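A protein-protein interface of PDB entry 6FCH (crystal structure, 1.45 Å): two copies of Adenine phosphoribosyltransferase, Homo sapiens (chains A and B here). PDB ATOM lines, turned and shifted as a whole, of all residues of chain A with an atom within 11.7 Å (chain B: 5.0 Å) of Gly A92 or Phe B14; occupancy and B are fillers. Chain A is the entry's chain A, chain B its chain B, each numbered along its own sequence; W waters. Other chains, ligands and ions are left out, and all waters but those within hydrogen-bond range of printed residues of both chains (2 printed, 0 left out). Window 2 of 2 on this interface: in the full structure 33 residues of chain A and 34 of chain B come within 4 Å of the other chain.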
ATOM      1  N   LEU A  83      -5.811 -18.133  -4.292  1.00  0.00           N
ATOM      2  CA  LEU A  83      -4.934 -17.404  -3.400  1.00  0.00           C
ATOM      3  C   LEU A  83      -5.013 -17.939  -1.990  1.00  0.00           C
ATOM      4  O   LEU A  83      -6.098 -18.198  -1.476  1.00  0.00           O
ATOM      5  CB  LEU A  83      -5.317 -15.931  -3.352  1.00  0.00           C
ATOM      6  CG  LEU A  83      -5.384 -15.213  -4.684  1.00  0.00           C
ATOM      7  CD1 LEU A  83      -5.662 -13.740  -4.455  1.00  0.00           C
ATOM      8  CD2 LEU A  83      -4.101 -15.399  -5.468  1.00  0.00           C
ATOM      9  N   ARG A  85      -3.558 -16.464   1.586  1.00  0.00           N
ATOM     10  CA  ARG A  85      -3.022 -15.203   2.058  1.00  0.00           C
ATOM     11  C   ARG A  85      -2.600 -15.231   3.512  1.00  0.00           C
ATOM     12  O   ARG A  85      -3.038 -16.080   4.285  1.00  0.00           O
ATOM     13  CB  ARG A  85      -4.061 -14.099   1.867  1.00  0.00           C
ATOM     14  CG  ARG A  85      -4.388 -13.822   0.410  1.00  0.00           C
ATOM     15  CD  ARG A  85      -4.429 -12.333   0.117  1.00  0.00           C
ATOM     16  NE  ARG A  85      -3.179 -11.696   0.498  1.00  0.00           N
ATOM     17  CZ  ARG A  85      -2.972 -10.384   0.486  1.00  0.00           C
ATOM     18  NH1 ARG A  85      -3.932  -9.566   0.080  1.00  0.00           N
ATOM     19  NH2 ARG A  85      -1.799  -9.897   0.865  1.00  0.00           N
ATOM     20  N   LYS A  86      -1.761 -14.278   3.891  1.00  0.00           N
ATOM     21  CA  LYS A  86      -1.542 -14.012   5.299  1.00  0.00           C
ATOM     22  C   LYS A  86      -2.877 -13.606   5.906  1.00  0.00           C
ATOM     23  O   LYS A  86      -3.695 -12.927   5.287  1.00  0.00           O
ATOM     24  CB  LYS A  86      -0.491 -12.916   5.493  1.00  0.00           C
ATOM     25  CG  LYS A  86       0.853 -13.251   4.865  1.00  0.00           C
ATOM     26  CD  LYS A  86       1.505 -14.453   5.522  1.00  0.00           C
ATOM     27  CE  LYS A  86       2.636 -15.014   4.668  1.00  0.00           C
ATOM     28  NZ  LYS A  86       3.772 -14.062   4.536  1.00  0.00           N
ATOM     29  N   ARG A  87      -3.114 -14.033   7.133  1.00  0.00           N
ATOM     30  CA  ARG A  87      -4.413 -13.827   7.721  1.00  0.00           C
ATOM     31  C   ARG A  87      -4.767 -12.351   7.851  1.00  0.00           C
ATOM     32  O   ARG A  87      -3.907 -11.519   8.155  1.00  0.00           O
ATOM     33  CB  ARG A  87      -4.498 -14.492   9.084  1.00  0.00           C
ATOM     34  CG  ARG A  87      -5.874 -14.347   9.690  1.00  0.00           C
ATOM     35  CD  ARG A  87      -6.007 -15.141  10.953  1.00  0.00           C
ATOM     36  NE  ARG A  87      -7.280 -14.857  11.590  1.00  0.00           N
ATOM     37  CZ  ARG A  87      -7.552 -15.131  12.851  1.00  0.00           C
ATOM     38  NH1 ARG A  87      -8.744 -14.824  13.358  1.00  0.00           N
ATOM     39  NH2 ARG A  87      -6.641 -15.718  13.596  1.00  0.00           N
ATOM     40  N   GLY A  88      -6.037 -12.048   7.599  1.00  0.00           N
ATOM     41  CA  GLY A  88      -6.583 -10.694   7.770  1.00  0.00           C
ATOM     42  C   GLY A  88      -6.825  -9.936   6.482  1.00  0.00           C
ATOM     43  O   GLY A  88      -7.331  -8.813   6.509  1.00  0.00           O
ATOM     44  N   LYS A  89      -6.486 -10.548   5.356  1.00  0.00           N
ATOM     45  CA  LYS A  89      -6.467  -9.839   4.081  1.00  0.00           C
ATOM     46  C   LYS A  89      -7.669 -10.172   3.199  1.00  0.00           C
ATOM     47  O   LYS A  89      -8.062  -9.377   2.338  1.00  0.00           O
ATOM     48  CB  LYS A  89      -5.182 -10.181   3.329  1.00  0.00           C
ATOM     49  CG  LYS A  89      -3.901  -9.885   4.100  1.00  0.00           C
ATOM     50  CD  LYS A  89      -3.369  -8.493   3.811  1.00  0.00           C
ATOM     51  CE  LYS A  89      -4.363  -7.413   4.203  1.00  0.00           C
ATOM     52  NZ  LYS A  89      -3.934  -6.060   3.738  1.00  0.00           N
ATOM     53  N   LEU A  90      -8.240 -11.348   3.393  1.00  0.00           N
ATOM     54  CA  LEU A  90      -9.296 -11.842   2.519  1.00  0.00           C
ATOM     55  C   LEU A  90     -10.672 -11.526   3.067  1.00  0.00           C
ATOM     56  O   LEU A  90     -10.899 -11.675   4.263  1.00  0.00           O
ATOM     57  CB  LEU A  90      -9.159 -13.351   2.363  1.00  0.00           C
ATOM     58  CG  LEU A  90      -7.991 -13.805   1.494  1.00  0.00           C
ATOM     59  CD1 LEU A  90      -7.790 -15.303   1.677  1.00  0.00           C
ATOM     60  CD2 LEU A  90      -8.233 -13.457   0.038  1.00  0.00           C
ATOM     61  N   PRO A  91     -11.609 -11.105   2.186  1.00  0.00           N
ATOM     62  CA  PRO A  91     -13.000 -10.919   2.564  1.00  0.00           C
ATOM     63  C   PRO A  91     -13.759 -12.227   2.531  1.00  0.00           C
ATOM     64  O   PRO A  91     -13.289 -13.209   1.934  1.00  0.00           O
ATOM     65  CB  PRO A  91     -13.525  -9.996   1.463  1.00  0.00           C
ATOM     66  CG  PRO A  91     -12.758 -10.432   0.257  1.00  0.00           C
ATOM     67  CD  PRO A  91     -11.380 -10.747   0.770  1.00  0.00           C
ATOM     68  N   GLY A  92     -14.928 -12.252   3.156  1.00  0.00           N
ATOM     69  CA  GLY A  92     -15.749 -13.444   3.144  1.00  0.00           C
ATOM     70  C   GLY A  92     -15.330 -14.433   4.210  1.00  0.00           C
ATOM     71  O   GLY A  92     -14.339 -14.232   4.902  1.00  0.00           O
ATOM     72  N   PRO A  93     -16.089 -15.516   4.347  1.00  0.00           N
ATOM     73  CA  PRO A  93     -15.760 -16.545   5.324  1.00  0.00           C
ATOM     74  C   PRO A  93     -14.426 -17.189   5.006  1.00  0.00           C
ATOM     75  O   PRO A  93     -14.160 -17.493   3.846  1.00  0.00           O
ATOM     76  CB  PRO A  93     -16.899 -17.552   5.165  1.00  0.00           C
ATOM     77  CG  PRO A  93     -18.039 -16.746   4.671  1.00  0.00           C
ATOM     78  CD  PRO A  93     -17.409 -15.738   3.745  1.00  0.00           C
ATOM     79  N   THR A  94     -13.603 -17.388   6.020  1.00  0.00           N
ATOM     80  CA  THR A  94     -12.274 -17.940   5.817  1.00  0.00           C
ATOM     81  C   THR A  94     -11.974 -19.026   6.831  1.00  0.00           C
ATOM     82  O   THR A  94     -12.686 -19.183   7.828  1.00  0.00           O
ATOM     83  CB  THR A  94     -11.192 -16.868   5.970  1.00  0.00           C
ATOM     84  OG1 THR A  94     -11.230 -16.339   7.298  1.00  0.00           O
ATOM     85  CG2 THR A  94     -11.394 -15.740   4.971  1.00  0.00           C
ATOM     86  N   LEU A  95     -10.934 -19.791   6.523  1.00  0.00           N
ATOM     87  CA  LEU A  95     -10.274 -20.703   7.439  1.00  0.00           C
ATOM     88  C   LEU A  95      -8.860 -20.235   7.549  1.00  0.00           C
ATOM     89  O   LEU A  95      -8.321 -19.700   6.594  1.00  0.00           O
ATOM     90  CB  LEU A  95     -10.161 -22.095   6.850  1.00  0.00           C
ATOM     91  CG  LEU A  95     -11.272 -22.802   6.168  1.00  0.00           C
ATOM     92  CD1 LEU A  95     -10.706 -24.185   5.835  1.00  0.00           C
ATOM     93  CD2 LEU A  95     -12.403 -22.851   7.174  1.00  0.00           C
ATOM     94  N   TRP A  96      -8.219 -20.493   8.668  1.00  0.00           N
ATOM     95  CA  TRP A  96      -6.816 -20.137   8.816  1.00  0.00           C
ATOM     96  C   TRP A  96      -6.007 -21.220   9.523  1.00  0.00           C
ATOM     97  O   TRP A  96      -6.557 -22.125  10.159  1.00  0.00           O
ATOM     98  CB  TRP A  96      -6.664 -18.781   9.516  1.00  0.00           C
ATOM     99  CG  TRP A  96      -7.273 -18.711  10.832  1.00  0.00           C
ATOM    100  CD1 TRP A  96      -6.703 -19.072  12.002  1.00  0.00           C
ATOM    101  CD2 TRP A  96      -8.575 -18.225  11.150  1.00  0.00           C
ATOM    102  NE1 TRP A  96      -7.578 -18.862  13.036  1.00  0.00           N
ATOM    103  CE2 TRP A  96      -8.731 -18.338  12.538  1.00  0.00           C
ATOM    104  CE3 TRP A  96      -9.626 -17.715  10.396  1.00  0.00           C
ATOM    105  CZ2 TRP A  96      -9.896 -17.956  13.189  1.00  0.00           C
ATOM    106  CZ3 TRP A  96     -10.766 -17.334  11.040  1.00  0.00           C
ATOM    107  CH2 TRP A  96     -10.894 -17.463  12.426  1.00  0.00           C
ATOM    108  N   LEU A 108      -1.720 -18.457   7.767  1.00  0.00           N
ATOM    109  CA  LEU A 108      -2.233 -18.354   6.420  1.00  0.00           C
ATOM    110  C   LEU A 108      -3.742 -18.527   6.459  1.00  0.00           C
ATOM    111  O   LEU A 108      -4.294 -19.060   7.428  1.00  0.00           O
ATOM    112  CB  LEU A 108      -1.628 -19.412   5.496  1.00  0.00           C
ATOM    113  CG  LEU A 108      -0.133 -19.334   5.204  1.00  0.00           C
ATOM    114  CD1 LEU A 108       0.234 -20.335   4.121  1.00  0.00           C
ATOM    115  CD2 LEU A 108       0.259 -17.930   4.788  1.00  0.00           C
ATOM    116  N   GLU A 109      -4.398 -18.103   5.391  1.00  0.00           N
ATOM    117  CA  GLU A 109      -5.852 -18.071   5.350  1.00  0.00           C
ATOM    118  C   GLU A 109      -6.357 -18.289   3.928  1.00  0.00           C
ATOM    119  O   GLU A 109      -5.685 -17.942   2.951  1.00  0.00           O
ATOM    120  CB  GLU A 109      -6.326 -16.731   5.906  1.00  0.00           C
ATOM    121  CG  GLU A 109      -7.812 -16.552   6.052  1.00  0.00           C
ATOM    122  CD  GLU A 109      -8.153 -15.302   6.848  1.00  0.00           C
ATOM    123  OE1 GLU A 109      -8.952 -15.390   7.819  1.00  0.00           O
ATOM    124  OE2 GLU A 109      -7.573 -14.237   6.537  1.00  0.00           O
ATOM    125  N   ILE A 110      -7.517 -18.901   3.807  1.00  0.00           N
ATOM    126  CA  ILE A 110      -8.104 -19.165   2.514  1.00  0.00           C
ATOM    127  C   ILE A 110      -9.609 -18.951   2.636  1.00  0.00           C
ATOM    128  O   ILE A 110     -10.186 -19.180   3.708  1.00  0.00           O
ATOM    129  CB  ILE A 110      -7.787 -20.598   2.052  1.00  0.00           C
ATOM    130  CG1 ILE A 110      -8.040 -20.751   0.554  1.00  0.00           C
ATOM    131  CG2 ILE A 110      -8.605 -21.620   2.833  1.00  0.00           C
ATOM    132  CD1 ILE A 110      -7.520 -22.064   0.020  1.00  0.00           C
ATOM    133  N   GLN A 111     -10.240 -18.461   1.577  1.00  0.00           N
ATOM    134  CA  GLN A 111     -11.692 -18.328   1.572  1.00  0.00           C
ATOM    135  C   GLN A 111     -12.315 -19.718   1.580  1.00  0.00           C
ATOM    136  O   GLN A 111     -11.832 -20.624   0.924  1.00  0.00           O
ATOM    137  CB  GLN A 111     -12.165 -17.511   0.366  1.00  0.00           C
ATOM    138  CG  GLN A 111     -11.792 -16.037   0.470  1.00  0.00           C
ATOM    139  CD  GLN A 111     -12.008 -15.243  -0.812  1.00  0.00           C
ATOM    140  OE1 GLN A 111     -11.903 -15.766  -1.924  1.00  0.00           O
ATOM    141  NE2 GLN A 111     -12.297 -13.966  -0.658  1.00  0.00           N
ATOM    142  N   LYS A 112     -13.374 -19.879   2.357  1.00  0.00           N
ATOM    143  CA  LYS A 112     -14.059 -21.161   2.458  1.00  0.00           C
ATOM    144  C   LYS A 112     -14.563 -21.649   1.110  1.00  0.00           C
ATOM    145  O   LYS A 112     -14.741 -22.850   0.920  1.00  0.00           O
ATOM    146  CB  LYS A 112     -15.232 -21.065   3.427  1.00  0.00           C
ATOM    147  CG  LYS A 112     -14.848 -20.903   4.881  1.00  0.00           C
ATOM    148  CD  LYS A 112     -16.057 -21.094   5.771  1.00  0.00           C
ATOM    149  CE  LYS A 112     -15.741 -20.845   7.224  1.00  0.00           C
ATOM    150  NZ  LYS A 112     -16.904 -21.217   8.080  1.00  0.00           N
ATOM    151  N   ASP A 113     -14.839 -20.719   0.195  1.00  0.00           N
ATOM    152  CA  ASP A 113     -15.356 -21.080  -1.121  1.00  0.00           C
ATOM    153  C   ASP A 113     -14.278 -21.105  -2.200  1.00  0.00           C
ATOM    154  O   ASP A 113     -14.593 -21.145  -3.386  1.00  0.00           O
ATOM    155  CB  ASP A 113     -16.512 -20.146  -1.533  1.00  0.00           C
ATOM    156  CG  ASP A 113     -16.050 -18.728  -1.844  1.00  0.00           C
ATOM    157  OD1 ASP A 113     -14.878 -18.406  -1.610  1.00  0.00           O
ATOM    158  OD2 ASP A 113     -16.885 -17.923  -2.319  1.00  0.00           O
ATOM    159  N   ALA A 114     -13.010 -21.140  -1.801  1.00  0.00           N
ATOM    160  CA  ALA A 114     -11.919 -21.079  -2.785  1.00  0.00           C
ATOM    161  C   ALA A 114     -11.871 -22.327  -3.678  1.00  0.00           C
ATOM    162  O   ALA A 114     -11.534 -22.239  -4.860  1.00  0.00           O
ATOM    163  CB  ALA A 114     -10.584 -20.885  -2.089  1.00  0.00           C
ATOM    164  N   LEU A 144     -10.574 -27.886   3.025  1.00  0.00           N
ATOM    165  CA  LEU A 144     -11.591 -27.681   1.986  1.00  0.00           C
ATOM    166  C   LEU A 144     -11.891 -28.965   1.218  1.00  0.00           C
ATOM    167  O   LEU A 144     -12.661 -28.949   0.260  1.00  0.00           O
ATOM    168  CB  LEU A 144     -11.151 -26.614   0.990  1.00  0.00           C
ATOM    169  CG  LEU A 144     -10.996 -25.205   1.554  1.00  0.00           C
ATOM    170  CD1 LEU A 144     -10.617 -24.254   0.435  1.00  0.00           C
ATOM    171  CD2 LEU A 144     -12.263 -24.741   2.255  1.00  0.00           C
ATOM    172  N   ARG B  12     -15.552  -9.316  -7.464  1.00  0.00           N
ATOM    173  CA  ARG B  12     -16.543  -9.612  -6.449  1.00  0.00           C
ATOM    174  C   ARG B  12     -16.479  -8.525  -5.382  1.00  0.00           C
ATOM    175  O   ARG B  12     -15.420  -8.247  -4.831  1.00  0.00           O
ATOM    176  CB  ARG B  12     -16.254 -10.973  -5.828  1.00  0.00           C
ATOM    177  CG  ARG B  12     -17.337 -11.483  -4.910  1.00  0.00           C
ATOM    178  CD  ARG B  12     -17.095 -12.942  -4.559  1.00  0.00           C
ATOM    179  NE  ARG B  12     -15.670 -13.229  -4.400  1.00  0.00           N
ATOM    180  CZ  ARG B  12     -15.181 -14.367  -3.921  1.00  0.00           C
ATOM    181  NH1 ARG B  12     -16.006 -15.332  -3.535  1.00  0.00           N
ATOM    182  NH2 ARG B  12     -13.863 -14.537  -3.818  1.00  0.00           N
ATOM    183  N   SER B  13     -17.615  -7.890  -5.125  1.00  0.00           N
ATOM    184  CA  SER B  13     -17.649  -6.720  -4.254  1.00  0.00           C
ATOM    185  C   SER B  13     -18.284  -7.070  -2.922  1.00  0.00           C
ATOM    186  O   SER B  13     -19.459  -7.444  -2.861  1.00  0.00           O
ATOM    187  CB  SER B  13     -18.409  -5.581  -4.929  1.00  0.00           C
ATOM    188  OG  SER B  13     -17.715  -5.136  -6.082  1.00  0.00           O
ATOM    189  N   PHE B  14     -17.478  -7.009  -1.863  1.00  0.00           N
ATOM    190  CA  PHE B  14     -17.926  -7.344  -0.514  1.00  0.00           C
ATOM    191  C   PHE B  14     -18.206  -6.086   0.291  1.00  0.00           C
ATOM    192  O   PHE B  14     -17.302  -5.292   0.528  1.00  0.00           O
ATOM    193  CB  PHE B  14     -16.856  -8.137   0.233  1.00  0.00           C
ATOM    194  CG  PHE B  14     -16.664  -9.522  -0.267  1.00  0.00           C
ATOM    195  CD1 PHE B  14     -15.794  -9.775  -1.304  1.00  0.00           C
ATOM    196  CD2 PHE B  14     -17.324 -10.585   0.328  1.00  0.00           C
ATOM    197  CE1 PHE B  14     -15.601 -11.055  -1.767  1.00  0.00           C
ATOM    198  CE2 PHE B  14     -17.136 -11.877  -0.136  1.00  0.00           C
ATOM    199  CZ  PHE B  14     -16.277 -12.107  -1.185  1.00  0.00           C
ATOM    200  N   PRO B  15     -19.447  -5.924   0.757  1.00  0.00           N
ATOM    201  CA  PRO B  15     -19.772  -4.763   1.589  1.00  0.00           C
ATOM    202  C   PRO B  15     -19.204  -4.879   2.996  1.00  0.00           C
ATOM    203  O   PRO B  15     -19.019  -5.981   3.509  1.00  0.00           O
ATOM    204  CB  PRO B  15     -21.296  -4.779   1.634  1.00  0.00           C
ATOM    205  CG  PRO B  15     -21.642  -6.215   1.484  1.00  0.00           C
ATOM    206  CD  PRO B  15     -20.601  -6.821   0.580  1.00  0.00           C
ATOM    207  N   ASP B  16     -18.911  -3.734   3.605  1.00  0.00           N
ATOM    208  CA  ASP B  16     -18.523  -3.667   5.010  1.00  0.00           C
ATOM    209  C   ASP B  16     -17.274  -4.464   5.335  1.00  0.00           C
ATOM    210  O   ASP B  16     -17.167  -5.052   6.405  1.00  0.00           O
ATOM    211  CB  ASP B  16     -19.681  -4.128   5.888  1.00  0.00           C
ATOM    212  CG  ASP B  16     -20.955  -3.395   5.575  1.00  0.00           C
ATOM    213  OD1 ASP B  16     -20.922  -2.139   5.478  1.00  0.00           O
ATOM    214  OD2 ASP B  16     -21.994  -4.059   5.383  1.00  0.00           O
ATOM    215  N   PHE B  17     -16.315  -4.456   4.415  1.00  0.00           N
ATOM    216  CA  PHE B  17     -15.026  -5.081   4.657  1.00  0.00           C
ATOM    217  C   PHE B  17     -13.935  -4.108   4.249  1.00  0.00           C
ATOM    218  O   PHE B  17     -13.930  -3.651   3.116  1.00  0.00           O
ATOM    219  CB  PHE B  17     -14.885  -6.393   3.875  1.00  0.00           C
ATOM    220  CG  PHE B  17     -13.638  -7.134   4.208  1.00  0.00           C
ATOM    221  CD1 PHE B  17     -13.576  -7.940   5.332  1.00  0.00           C
ATOM    222  CD2 PHE B  17     -12.496  -6.966   3.444  1.00  0.00           C
ATOM    223  CE1 PHE B  17     -12.406  -8.584   5.671  1.00  0.00           C
ATOM    224  CE2 PHE B  17     -11.328  -7.612   3.776  1.00  0.00           C
ATOM    225  CZ  PHE B  17     -11.282  -8.423   4.889  1.00  0.00           C
ATOM    226  N   VAL B  22     -17.545   0.398   3.818  1.00  0.00           N
ATOM    227  CA  VAL B  22     -16.509   0.245   2.802  1.00  0.00           C
ATOM    228  C   VAL B  22     -16.758  -1.008   1.990  1.00  0.00           C
ATOM    229  O   VAL B  22     -16.981  -2.079   2.550  1.00  0.00           O
ATOM    230  CB  VAL B  22     -15.121   0.131   3.453  1.00  0.00           C
ATOM    231  CG1 VAL B  22     -14.030   0.083   2.395  1.00  0.00           C
ATOM    232  CG2 VAL B  22     -14.885   1.302   4.402  1.00  0.00           C
ATOM    233  N   VAL B  23     -16.725  -0.866   0.670  1.00  0.00           N
ATOM    234  CA  VAL B  23     -16.861  -2.003  -0.231  1.00  0.00           C
ATOM    235  C   VAL B  23     -15.509  -2.474  -0.733  1.00  0.00           C
ATOM    236  O   VAL B  23     -14.742  -1.704  -1.310  1.00  0.00           O
ATOM    237  CB  VAL B  23     -17.762  -1.661  -1.431  1.00  0.00           C
ATOM    238  CG1 VAL B  23     -17.911  -2.850  -2.348  1.00  0.00           C
ATOM    239  CG2 VAL B  23     -19.129  -1.219  -0.935  1.00  0.00           C
ATOM    240  N   PHE B  24     -15.225  -3.748  -0.510  1.00  0.00           N
ATOM    241  CA  PHE B  24     -13.969  -4.339  -0.924  1.00  0.00           C
ATOM    242  C   PHE B  24     -14.127  -4.955  -2.296  1.00  0.00           C
ATOM    243  O   PHE B  24     -14.988  -5.784  -2.503  1.00  0.00           O
ATOM    244  CB  PHE B  24     -13.550  -5.413   0.086  1.00  0.00           C
ATOM    245  CG  PHE B  24     -12.172  -5.962  -0.137  1.00  0.00           C
ATOM    246  CD1 PHE B  24     -11.967  -7.027  -0.993  1.00  0.00           C
ATOM    247  CD2 PHE B  24     -11.088  -5.440   0.550  1.00  0.00           C
ATOM    248  CE1 PHE B  24     -10.702  -7.547  -1.186  1.00  0.00           C
ATOM    249  CE2 PHE B  24      -9.818  -5.958   0.360  1.00  0.00           C
ATOM    250  CZ  PHE B  24      -9.624  -7.003  -0.518  1.00  0.00           C
ATOM    251  N   ASP B  26     -12.814  -7.466  -4.648  1.00  0.00           N
ATOM    252  CA  ASP B  26     -12.003  -8.669  -4.640  1.00  0.00           C
ATOM    253  C   ASP B  26     -11.713  -9.102  -6.080  1.00  0.00           C
ATOM    254  O   ASP B  26     -12.634  -9.385  -6.854  1.00  0.00           O
ATOM    255  CB  ASP B  26     -12.757  -9.762  -3.883  1.00  0.00           C
ATOM    256  CG  ASP B  26     -11.973 -11.064  -3.766  1.00  0.00           C
ATOM    257  OD1 ASP B  26     -10.757 -11.060  -4.010  1.00  0.00           O
ATOM    258  OD2 ASP B  26     -12.606 -12.081  -3.409  1.00  0.00           O
HETATM  259  O   HOH W   1     -13.016 -17.786  -3.241  1.00  0.00           O
HETATM  260  O   HOH W   2     -16.036 -15.797  -0.096  1.00  0.00           O
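The guanidinium group (NH2) of Arg B12 lies within hydrogen-bond range of the side-chain amide oxygen (OE1) of Gln A111 (3.0 Å). The side-chain carboxylate (OD2) of Asp B26 is in hydrogen-bond range of the side-chain amide nitrogen (NE2) of Gln A111 (3.3 Å). The side-chain carboxylate (OD2) of Asp A113 lies within salt-bridge range of the guanidinium group (NH1) of Arg B12 (3.0 Å).
O of Pro A91 sits at hydrogen-bond distance from NE2 of Gln A111 (2.9 Å). OD2 of Asp B26 is in salt-bridge range of NH2 of Arg B12. O of Phe B14 sits at hydrogen-bond distance from N of Phe B24 (2.8 Å). N of Phe B17 is in hydrogen-bond range of O of Val B22 (3.1 Å).
Lys A89 touches Phe B17. Leu A90 touches Phe B17 (O to CZ, 3.3 Å). CD1 of Phe B14 touches CG of Pro A91, at 3.5 Å. Pro A91 touches Phe B17. Phe B24 touches Pro A91 (CD1 to CG, 3.7 Å). Phe B14 touches Gly A92 (CE2 to CA, 3.9 Å).
Gly A92 touches just one residue of chain B: Phe B14 (3.9 Å). Of chain A, only Gln A111 (3.0 Å) and Asp A113 (3.0 Å) come within 4 Å of Arg B12. Ser B13 touches none of the printed residues of chain A. Pro B15 touches none of the printed residues of chain A. No residue of chain A comes within 4 Å of Asp B16. Asp B26 touches one residue of chain A. Of the printed residues of chain B, Gln A111 touches Arg B12 and Asp B26. Printed residues of chain A within 4 Å of Phe B17: Lys A89 (3.98 Å), Leu A90 (3.3 Å) and Pro A91 (3.8 Å). Of the printed residues of chain B, Lys A89 touches Phe B17 (3.98 Å). Printed residues of chain B within 4 Å of Leu A90: Phe B17. Of the printed residues of chain B, Pro A91 touches Phe B14, Phe B17 and Phe B24. Ile A110 touches none of the printed residues of chain B. Lys A112 touches none of the printed residues of chain B. The nearest residue of chain A that does not touch Phe B14 is Gln A111 (4.4 Å). The nearest printed residue of chain A that does not touch Phe B17 is Gly A88 (4.3 Å).
Hydrophobic or aromatic side chains of chain A that line the printed part of chain B: Pro A91. Printed residues of chain B that touch a printed residue of chain A: Arg B12, Phe B14, Phe B17, Phe B24 and Asp B26. Hydrophobic or aromatic side chains of chain B within 4 Å of the printed part of chain A: Phe B14, Phe B17 and Phe B24. Among the printed residues, 9 pairs touch across the chains. Among the printed residues, Asp or Glu carboxylates within 4 Å of a Lys or Arg side-chain nitrogen of the other chain: Asp A113 with Arg B12.
No position is printed for both chains.
Water W1 lies within hydrogen-bond range of the side-chain carboxylate of Asp A113, the side-chain amide oxygen of Gln A111 and the guanidinium group of Arg B12. Water W2 lies within hydrogen-bond range of the side-chain carboxylate of Asp A113 and the guanidinium group of Arg B12.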
